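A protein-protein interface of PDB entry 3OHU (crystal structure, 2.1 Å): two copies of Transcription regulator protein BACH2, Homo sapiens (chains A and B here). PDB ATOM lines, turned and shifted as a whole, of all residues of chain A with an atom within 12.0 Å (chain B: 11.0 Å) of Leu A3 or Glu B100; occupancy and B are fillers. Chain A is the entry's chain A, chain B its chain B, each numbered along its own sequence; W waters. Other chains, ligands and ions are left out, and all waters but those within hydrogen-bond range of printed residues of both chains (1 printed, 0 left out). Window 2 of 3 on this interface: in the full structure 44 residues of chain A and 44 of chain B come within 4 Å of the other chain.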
ATOM      1  N   GLY A   1      -9.757  33.948 -28.560  1.00  0.00           N
ATOM      2  CA  GLY A   1      -9.932  34.065 -27.090  1.00  0.00           C
ATOM      3  C   GLY A   1     -10.609  32.859 -26.450  1.00  0.00           C
ATOM      4  O   GLY A   1     -11.711  32.988 -25.918  1.00  0.00           O
ATOM      5  N   PRO A   2      -9.953  31.674 -26.484  1.00  0.00           N
ATOM      6  CA  PRO A   2     -10.546  30.525 -25.812  1.00  0.00           C
ATOM      7  C   PRO A   2     -10.399  30.641 -24.292  1.00  0.00           C
ATOM      8  O   PRO A   2      -9.571  31.420 -23.796  1.00  0.00           O
ATOM      9  CB  PRO A   2      -9.730  29.328 -26.342  1.00  0.00           C
ATOM     10  CG  PRO A   2      -8.858  29.882 -27.480  1.00  0.00           C
ATOM     11  CD  PRO A   2      -8.660  31.329 -27.101  1.00  0.00           C
ATOM     12  N   LEU A   3     -11.220  29.886 -23.566  1.00  0.00           N
ATOM     13  CA  LEU A   3     -11.109  29.824 -22.116  1.00  0.00           C
ATOM     14  C   LEU A   3     -10.467  28.491 -21.789  1.00  0.00           C
ATOM     15  O   LEU A   3     -10.947  27.448 -22.230  1.00  0.00           O
ATOM     16  CB  LEU A   3     -12.483  29.959 -21.440  1.00  0.00           C
ATOM     17  CG  LEU A   3     -13.301  31.239 -21.681  1.00  0.00           C
ATOM     18  CD1 LEU A   3     -14.753  31.078 -21.213  1.00  0.00           C
ATOM     19  CD2 LEU A   3     -12.674  32.459 -21.007  1.00  0.00           C
ATOM     20  N   GLY A   4      -9.369  28.532 -21.047  1.00  0.00           N
ATOM     21  CA  GLY A   4      -8.648  27.324 -20.664  1.00  0.00           C
ATOM     22  C   GLY A   4      -7.603  26.989 -21.704  1.00  0.00           C
ATOM     23  O   GLY A   4      -7.617  27.524 -22.807  1.00  0.00           O
ATOM     24  N   SER A   5      -6.699  26.093 -21.357  1.00  0.00           N
ATOM     25  CA  SER A   5      -5.686  25.650 -22.290  1.00  0.00           C
ATOM     26  C   SER A   5      -6.283  24.741 -23.359  1.00  0.00           C
ATOM     27  O   SER A   5      -6.846  23.678 -23.040  1.00  0.00           O
ATOM     28  CB  SER A   5      -4.551  24.957 -21.539  1.00  0.00           C
ATOM     29  OG  SER A   5      -3.842  25.901 -20.778  1.00  0.00           O
ATOM     30  N   PRO A   6      -6.168  25.151 -24.644  1.00  0.00           N
ATOM     31  CA  PRO A   6      -6.632  24.277 -25.703  1.00  0.00           C
ATOM     32  C   PRO A   6      -5.588  23.189 -25.902  1.00  0.00           C
ATOM     33  O   PRO A   6      -4.743  23.273 -26.817  1.00  0.00           O
ATOM     34  CB  PRO A   6      -6.739  25.209 -26.933  1.00  0.00           C
ATOM     35  CG  PRO A   6      -5.976  26.474 -26.564  1.00  0.00           C
ATOM     36  CD  PRO A   6      -5.467  26.338 -25.169  1.00  0.00           C
ATOM     37  N   MET A   7      -5.658  22.180 -25.034  1.00  0.00           N
ATOM     38  CA  MET A   7      -4.641  21.143 -24.944  1.00  0.00           C
ATOM     39  C   MET A   7      -5.187  19.732 -25.156  1.00  0.00           C
ATOM     40  O   MET A   7      -4.411  18.762 -25.174  1.00  0.00           O
ATOM     41  CB  MET A   7      -3.938  21.215 -23.582  1.00  0.00           C
ATOM     42  CG  MET A   7      -4.885  20.988 -22.396  1.00  0.00           C
ATOM     43  SD  MET A   7      -4.023  20.857 -20.812  1.00  0.00           S
ATOM     44  CE  MET A   7      -3.664  19.097 -20.768  1.00  0.00           C
ATOM     45  N   TYR A   8      -6.503  19.601 -25.299  1.00  0.00           N
ATOM     46  CA  TYR A   8      -7.071  18.271 -25.489  1.00  0.00           C
ATOM     47  C   TYR A   8      -7.166  17.934 -26.966  1.00  0.00           C
ATOM     48  O   TYR A   8      -7.994  18.498 -27.704  1.00  0.00           O
ATOM     49  CB  TYR A   8      -8.399  18.116 -24.751  1.00  0.00           C
ATOM     50  CG  TYR A   8      -8.251  18.502 -23.290  1.00  0.00           C
ATOM     51  CD1 TYR A   8      -7.444  17.745 -22.432  1.00  0.00           C
ATOM     52  CD2 TYR A   8      -8.869  19.650 -22.783  1.00  0.00           C
ATOM     53  CE1 TYR A   8      -7.282  18.098 -21.116  1.00  0.00           C
ATOM     54  CE2 TYR A   8      -8.713  20.014 -21.463  1.00  0.00           C
ATOM     55  CZ  TYR A   8      -7.912  19.234 -20.633  1.00  0.00           C
ATOM     56  OH  TYR A   8      -7.749  19.577 -19.325  1.00  0.00           O
ATOM     57  N   VAL A   9      -6.316  17.002 -27.382  1.00  0.00           N
ATOM     58  CA  VAL A   9      -6.111  16.735 -28.799  1.00  0.00           C
ATOM     59  C   VAL A   9      -6.588  15.355 -29.290  1.00  0.00           C
ATOM     60  O   VAL A   9      -6.444  14.320 -28.608  1.00  0.00           O
ATOM     61  CB  VAL A   9      -4.620  16.981 -29.198  1.00  0.00           C
ATOM     62  CG1 VAL A   9      -3.690  15.846 -28.703  1.00  0.00           C
ATOM     63  CG2 VAL A   9      -4.483  17.202 -30.710  1.00  0.00           C
ATOM     64  N   THR B  79     -25.523  22.454 -30.555  1.00  0.00           N
ATOM     65  CA  THR B  79     -25.148  23.843 -30.251  1.00  0.00           C
ATOM     66  C   THR B  79     -24.016  24.283 -31.171  1.00  0.00           C
ATOM     67  O   THR B  79     -23.290  23.435 -31.714  1.00  0.00           O
ATOM     68  CB  THR B  79     -24.668  24.013 -28.795  1.00  0.00           C
ATOM     69  OG1 THR B  79     -23.406  23.347 -28.626  1.00  0.00           O
ATOM     70  CG2 THR B  79     -25.686  23.436 -27.808  1.00  0.00           C
ATOM     71  N   ALA B  80     -23.872  25.604 -31.324  1.00  0.00           N
ATOM     72  CA  ALA B  80     -22.799  26.207 -32.121  1.00  0.00           C
ATOM     73  C   ALA B  80     -21.407  25.919 -31.549  1.00  0.00           C
ATOM     74  O   ALA B  80     -20.483  25.597 -32.302  1.00  0.00           O
ATOM     75  CB  ALA B  80     -23.035  27.721 -32.275  1.00  0.00           C
ATOM     76  N   ARG B  81     -21.278  25.997 -30.220  1.00  0.00           N
ATOM     77  CA  ARG B  81     -20.020  25.709 -29.491  1.00  0.00           C
ATOM     78  C   ARG B  81     -19.476  24.292 -29.693  1.00  0.00           C
ATOM     79  O   ARG B  81     -18.255  24.098 -29.776  1.00  0.00           O
ATOM     80  CB  ARG B  81     -20.184  25.984 -27.983  1.00  0.00           C
ATOM     81  CG  ARG B  81     -19.063  25.395 -27.094  1.00  0.00           C
ATOM     82  CD  ARG B  81     -19.078  25.933 -25.656  1.00  0.00           C
ATOM     83  NE  ARG B  81     -18.839  27.376 -25.649  1.00  0.00           N
ATOM     84  CZ  ARG B  81     -18.909  28.163 -24.581  1.00  0.00           C
ATOM     85  NH1 ARG B  81     -19.202  27.661 -23.373  1.00  0.00           N
ATOM     86  NH2 ARG B  81     -18.676  29.464 -24.727  1.00  0.00           N
ATOM     87  N   GLY B  82     -20.371  23.305 -29.737  1.00  0.00           N
ATOM     88  CA  GLY B  82     -19.968  21.905 -29.968  1.00  0.00           C
ATOM     89  C   GLY B  82     -19.818  21.560 -31.437  1.00  0.00           C
ATOM     90  O   GLY B  82     -18.998  20.686 -31.813  1.00  0.00           O
ATOM     91  N   PHE B  83     -20.628  22.210 -32.275  1.00  0.00           N
ATOM     92  CA  PHE B  83     -20.626  21.909 -33.718  1.00  0.00           C
ATOM     93  C   PHE B  83     -19.398  22.455 -34.485  1.00  0.00           C
ATOM     94  O   PHE B  83     -18.853  21.766 -35.322  1.00  0.00           O
ATOM     95  CB  PHE B  83     -21.938  22.347 -34.416  1.00  0.00           C
ATOM     96  CG  PHE B  83     -21.949  22.055 -35.900  1.00  0.00           C
ATOM     97  CD1 PHE B  83     -22.136  20.753 -36.363  1.00  0.00           C
ATOM     98  CD2 PHE B  83     -21.701  23.057 -36.825  1.00  0.00           C
ATOM     99  CE1 PHE B  83     -22.123  20.458 -37.741  1.00  0.00           C
ATOM    100  CE2 PHE B  83     -21.670  22.774 -38.206  1.00  0.00           C
ATOM    101  CZ  PHE B  83     -21.886  21.470 -38.657  1.00  0.00           C
ATOM    102  N   PRO B  85     -16.195  22.962 -33.834  1.00  0.00           N
ATOM    103  CA  PRO B  85     -15.006  22.116 -33.850  1.00  0.00           C
ATOM    104  C   PRO B  85     -15.192  20.808 -34.634  1.00  0.00           C
ATOM    105  O   PRO B  85     -14.253  20.327 -35.257  1.00  0.00           O
ATOM    106  CB  PRO B  85     -14.758  21.862 -32.355  1.00  0.00           C
ATOM    107  CG  PRO B  85     -15.207  23.172 -31.695  1.00  0.00           C
ATOM    108  CD  PRO B  85     -16.456  23.531 -32.485  1.00  0.00           C
ATOM    109  N   LEU B  96      -8.887  20.037 -31.329  1.00  0.00           N
ATOM    110  CA  LEU B  96      -8.071  20.564 -30.247  1.00  0.00           C
ATOM    111  C   LEU B  96      -8.991  21.459 -29.421  1.00  0.00           C
ATOM    112  O   LEU B  96      -9.427  22.508 -29.887  1.00  0.00           O
ATOM    113  CB  LEU B  96      -6.854  21.343 -30.769  1.00  0.00           C
ATOM    114  CG  LEU B  96      -5.720  21.749 -29.800  1.00  0.00           C
ATOM    115  CD1 LEU B  96      -5.041  20.539 -29.105  1.00  0.00           C
ATOM    116  CD2 LEU B  96      -4.669  22.561 -30.555  1.00  0.00           C
ATOM    117  N   LEU B  97      -9.305  20.995 -28.216  1.00  0.00           N
ATOM    118  CA  LEU B  97     -10.376  21.561 -27.405  1.00  0.00           C
ATOM    119  C   LEU B  97      -9.824  21.996 -26.042  1.00  0.00           C
ATOM    120  O   LEU B  97      -8.736  21.567 -25.615  1.00  0.00           O
ATOM    121  CB  LEU B  97     -11.478  20.499 -27.212  1.00  0.00           C
ATOM    122  CG  LEU B  97     -12.038  19.780 -28.460  1.00  0.00           C
ATOM    123  CD1 LEU B  97     -13.008  18.649 -28.098  1.00  0.00           C
ATOM    124  CD2 LEU B  97     -12.731  20.759 -29.459  1.00  0.00           C
ATOM    125  N   SER B  98     -10.571  22.851 -25.369  1.00  0.00           N
ATOM    126  CA  SER B  98     -10.284  23.172 -23.987  1.00  0.00           C
ATOM    127  C   SER B  98     -11.435  22.732 -23.095  1.00  0.00           C
ATOM    128  O   SER B  98     -12.430  22.165 -23.565  1.00  0.00           O
ATOM    129  CB  SER B  98     -10.053  24.679 -23.826  1.00  0.00           C
ATOM    130  OG  SER B  98     -11.276  25.390 -23.897  1.00  0.00           O
ATOM    131  N   ARG B  99     -11.296  23.006 -21.804  1.00  0.00           N
ATOM    132  CA  ARG B  99     -12.356  22.761 -20.835  1.00  0.00           C
ATOM    133  C   ARG B  99     -13.710  23.446 -21.146  1.00  0.00           C
ATOM    134  O   ARG B  99     -14.743  22.966 -20.696  1.00  0.00           O
ATOM    135  CB  ARG B  99     -11.896  23.153 -19.425  1.00  0.00           C
ATOM    136  CG  ARG B  99     -11.533  24.623 -19.256  1.00  0.00           C
ATOM    137  CD  ARG B  99     -11.042  24.911 -17.833  1.00  0.00           C
ATOM    138  NE  ARG B  99     -10.523  26.264 -17.697  1.00  0.00           N
ATOM    139  CZ  ARG B  99     -11.249  27.315 -17.340  1.00  0.00           C
ATOM    140  NH1 ARG B  99     -12.552  27.171 -17.084  1.00  0.00           N
ATOM    141  NH2 ARG B  99     -10.681  28.517 -17.243  1.00  0.00           N
ATOM    142  N   GLU B 100     -13.684  24.557 -21.882  1.00  0.00           N
ATOM    143  CA  GLU B 100     -14.898  25.320 -22.184  1.00  0.00           C
ATOM    144  C   GLU B 100     -15.809  24.575 -23.164  1.00  0.00           C
ATOM    145  O   GLU B 100     -17.031  24.674 -23.074  1.00  0.00           O
ATOM    146  CB  GLU B 100     -14.540  26.715 -22.716  1.00  0.00           C
ATOM    147  CG  GLU B 100     -15.685  27.755 -22.732  1.00  0.00           C
ATOM    148  CD  GLU B 100     -16.148  28.219 -21.338  1.00  0.00           C
ATOM    149  OE1 GLU B 100     -15.445  27.968 -20.327  1.00  0.00           O
ATOM    150  OE2 GLU B 100     -17.229  28.845 -21.256  1.00  0.00           O
ATOM    151  N   ASN B 101     -15.221  23.810 -24.078  1.00  0.00           N
ATOM    152  CA  ASN B 101     -16.009  23.194 -25.152  1.00  0.00           C
ATOM    153  C   ASN B 101     -15.972  21.672 -25.273  1.00  0.00           C
ATOM    154  O   ASN B 101     -16.796  21.113 -25.998  1.00  0.00           O
ATOM    155  CB  ASN B 101     -15.703  23.877 -26.506  1.00  0.00           C
ATOM    156  CG  ASN B 101     -14.263  23.677 -26.954  1.00  0.00           C
ATOM    157  OD1 ASN B 101     -13.430  23.122 -26.214  1.00  0.00           O
ATOM    158  ND2 ASN B 101     -13.959  24.120 -28.189  1.00  0.00           N
ATOM    159  N   ILE B 102     -15.056  21.002 -24.562  1.00  0.00           N
ATOM    160  CA  ILE B 102     -14.885  19.544 -24.731  1.00  0.00           C
ATOM    161  C   ILE B 102     -16.178  18.765 -24.467  1.00  0.00           C
ATOM    162  O   ILE B 102     -16.511  17.841 -25.216  1.00  0.00           O
ATOM    163  CB  ILE B 102     -13.664  18.927 -23.925  1.00  0.00           C
ATOM    164  CG1 ILE B 102     -13.452  17.439 -24.267  1.00  0.00           C
ATOM    165  CG2 ILE B 102     -13.806  19.112 -22.401  1.00  0.00           C
ATOM    166  CD1 ILE B 102     -12.023  16.905 -23.949  1.00  0.00           C
ATOM    167  N   ARG B 103     -16.920  19.143 -23.432  1.00  0.00           N
ATOM    168  CA  ARG B 103     -18.148  18.426 -23.113  1.00  0.00           C
ATOM    169  C   ARG B 103     -19.148  18.550 -24.272  1.00  0.00           C
ATOM    170  O   ARG B 103     -19.678  17.554 -24.781  1.00  0.00           O
ATOM    171  CB  ARG B 103     -18.744  18.946 -21.801  1.00  0.00           C
ATOM    172  CG  ARG B 103     -20.123  18.403 -21.440  1.00  0.00           C
ATOM    173  CD  ARG B 103     -20.092  16.904 -21.375  1.00  0.00           C
ATOM    174  NE  ARG B 103     -21.420  16.315 -21.271  1.00  0.00           N
ATOM    175  CZ  ARG B 103     -21.717  15.085 -21.684  1.00  0.00           C
ATOM    176  NH1 ARG B 103     -20.780  14.338 -22.238  1.00  0.00           N
ATOM    177  NH2 ARG B 103     -22.949  14.611 -21.546  1.00  0.00           N
ATOM    178  N   GLU B 104     -19.394  19.792 -24.669  1.00  0.00           N
ATOM    179  CA  GLU B 104     -20.337  20.106 -25.744  1.00  0.00           C
ATOM    180  C   GLU B 104     -19.968  19.439 -27.070  1.00  0.00           C
ATOM    181  O   GLU B 104     -20.855  18.999 -27.799  1.00  0.00           O
ATOM    182  CB  GLU B 104     -20.444  21.618 -25.909  1.00  0.00           C
ATOM    183  CG  GLU B 104     -21.436  22.264 -24.942  1.00  0.00           C
ATOM    184  CD  GLU B 104     -22.881  21.803 -25.196  1.00  0.00           C
ATOM    185  OE1 GLU B 104     -23.251  21.553 -26.372  1.00  0.00           O
ATOM    186  OE2 GLU B 104     -23.647  21.675 -24.217  1.00  0.00           O
ATOM    187  N   VAL B 105     -18.668  19.367 -27.377  1.00  0.00           N
ATOM    188  CA  VAL B 105     -18.221  18.713 -28.597  1.00  0.00           C
ATOM    189  C   VAL B 105     -18.507  17.214 -28.555  1.00  0.00           C
ATOM    190  O   VAL B 105     -19.052  16.675 -29.511  1.00  0.00           O
ATOM    191  CB  VAL B 105     -16.739  19.016 -28.951  1.00  0.00           C
ATOM    192  CG1 VAL B 105     -16.244  18.123 -30.082  1.00  0.00           C
ATOM    193  CG2 VAL B 105     -16.578  20.469 -29.357  1.00  0.00           C
ATOM    194  N   ILE B 106     -18.185  16.557 -27.438  1.00  0.00           N
ATOM    195  CA  ILE B 106     -18.477  15.128 -27.306  1.00  0.00           C
ATOM    196  C   ILE B 106     -19.985  14.869 -27.440  1.00  0.00           C
ATOM    197  O   ILE B 106     -20.400  13.968 -28.172  1.00  0.00           O
ATOM    198  CB  ILE B 106     -17.982  14.549 -25.967  1.00  0.00           C
ATOM    199  CG1 ILE B 106     -16.475  14.751 -25.821  1.00  0.00           C
ATOM    200  CG2 ILE B 106     -18.313  13.036 -25.874  1.00  0.00           C
ATOM    201  CD1 ILE B 106     -15.991  14.648 -24.363  1.00  0.00           C
ATOM    202  N   ARG B 107     -20.792  15.675 -26.754  1.00  0.00           N
ATOM    203  CA  ARG B 107     -22.248  15.489 -26.760  1.00  0.00           C
ATOM    204  C   ARG B 107     -22.809  15.670 -28.173  1.00  0.00           C
ATOM    205  O   ARG B 107     -23.626  14.859 -28.619  1.00  0.00           O
ATOM    206  CB  ARG B 107     -22.943  16.431 -25.774  1.00  0.00           C
ATOM    207  CG  ARG B 107     -24.419  16.069 -25.512  1.00  0.00           C
ATOM    208  CD  ARG B 107     -25.033  16.866 -24.351  1.00  0.00           C
ATOM    209  NE  ARG B 107     -25.048  18.304 -24.620  1.00  0.00           N
ATOM    210  CZ  ARG B 107     -25.894  18.921 -25.447  1.00  0.00           C
ATOM    211  NH1 ARG B 107     -26.828  18.246 -26.118  1.00  0.00           N
ATOM    212  NH2 ARG B 107     -25.803  20.232 -25.609  1.00  0.00           N
HETATM  213  O   HOH W   1      -8.506  23.719 -20.906  1.00  0.00           O
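No position is printed for both chains.
O of Leu A3 is in hydrogen-bond range of OG of Ser B98 (2.7 Å).
The backbone carbonyl oxygen (O) of Leu B97 is in hydrogen-bond range of the backbone NH (N) of Met A7, 3.2 Å away.
The backbone carbonyl oxygen (O) of Tyr A8 is in hydrogen-bond range of the backbone NH (N) of Leu B97, at 2.9 Å.
The guanidinium group of Arg B81 lies within salt-bridge range of the side-chain carboxylate of Glu B100 (3.1 Å).
N of Glu B100 sits close to OG of Ser B98, at 3.2 Å.
OD1 of Asn B101 lies close to O of Ser B98 (3.0 Å).
No residue of chain B comes within 4 Å of Gly A1.
Of the printed residues of chain B, Leu A3 touches Ser B98 (2.7 Å) and Glu B100 (3.2 Å).
Of chain B, only Ser B98 (3.9 Å) and Arg B99 (3.7 Å) come within 4 Å of Gly A4.
Printed residues of chain B within 4 Å of Pro A6: Leu B96 (3.5 Å), Leu B97 (3.4 Å) and Ser B98 (3.9 Å).
Thr B79 touches none of the printed residues of chain A.
Pro B85 touches none of the printed residues of chain A.
Of the printed residues of chain A, Leu B96 touches Pro A6, Tyr A8 and Val A9.
Printed residues of chain A within 4 Å of Ser B98: Leu A3 (2.7 Å), Gly A4 (3.9 Å), Ser A5 (3.5 Å), Pro A6 (3.9 Å) and Tyr A8 (3.98 Å).
Printed residues of chain A within 4 Å of Glu B100: Leu A3 (3.2 Å).
No residue of chain A comes within 4 Å of Asn B101.
The nearest printed residue of chain B that does not touch Leu A3 is Arg B99 (4.1 Å).
The nearest printed residue of chain A that does not touch Glu B100 is Gly A4 (5.7 Å).
Among the printed residues, pairs that only touch across the chains: Leu A3 with Glu B100, Tyr A8 with Leu B96, Pro A6 with Leu B97, Ser A5 with Ser B98, Pro A6 with Leu B96, Val A9 with Leu B96, Gly A4 with Arg B99, Ser A5 with Leu B97, Gly A4 with Ser B98, Tyr A8 with Ile B102, Pro A6 with Ser B98, Tyr A8 with Arg B99 and Tyr A8 with Ser B98.
Printed residues of chain B that touch a printed residue of chain A: Leu B96, Leu B97, Ser B98, Arg B99, Glu B100 and Ile B102.
Hydrophobic or aromatic side chains of chain A within 4 Å of the printed part of chain B: Leu A3, Tyr A8 and Val A9.
Along chain A the printed residues that touch a printed residue of chain B span positions 3 to 9.
Among the printed residues, no Asp or Glu carboxylate lies within 4 Å of a Lys or Arg side-chain nitrogen of the other chain.
Water W1 lies within hydrogen-bond range of the backbone carbonyl oxygen of Ser A5 and the backbone NH of Arg B99.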
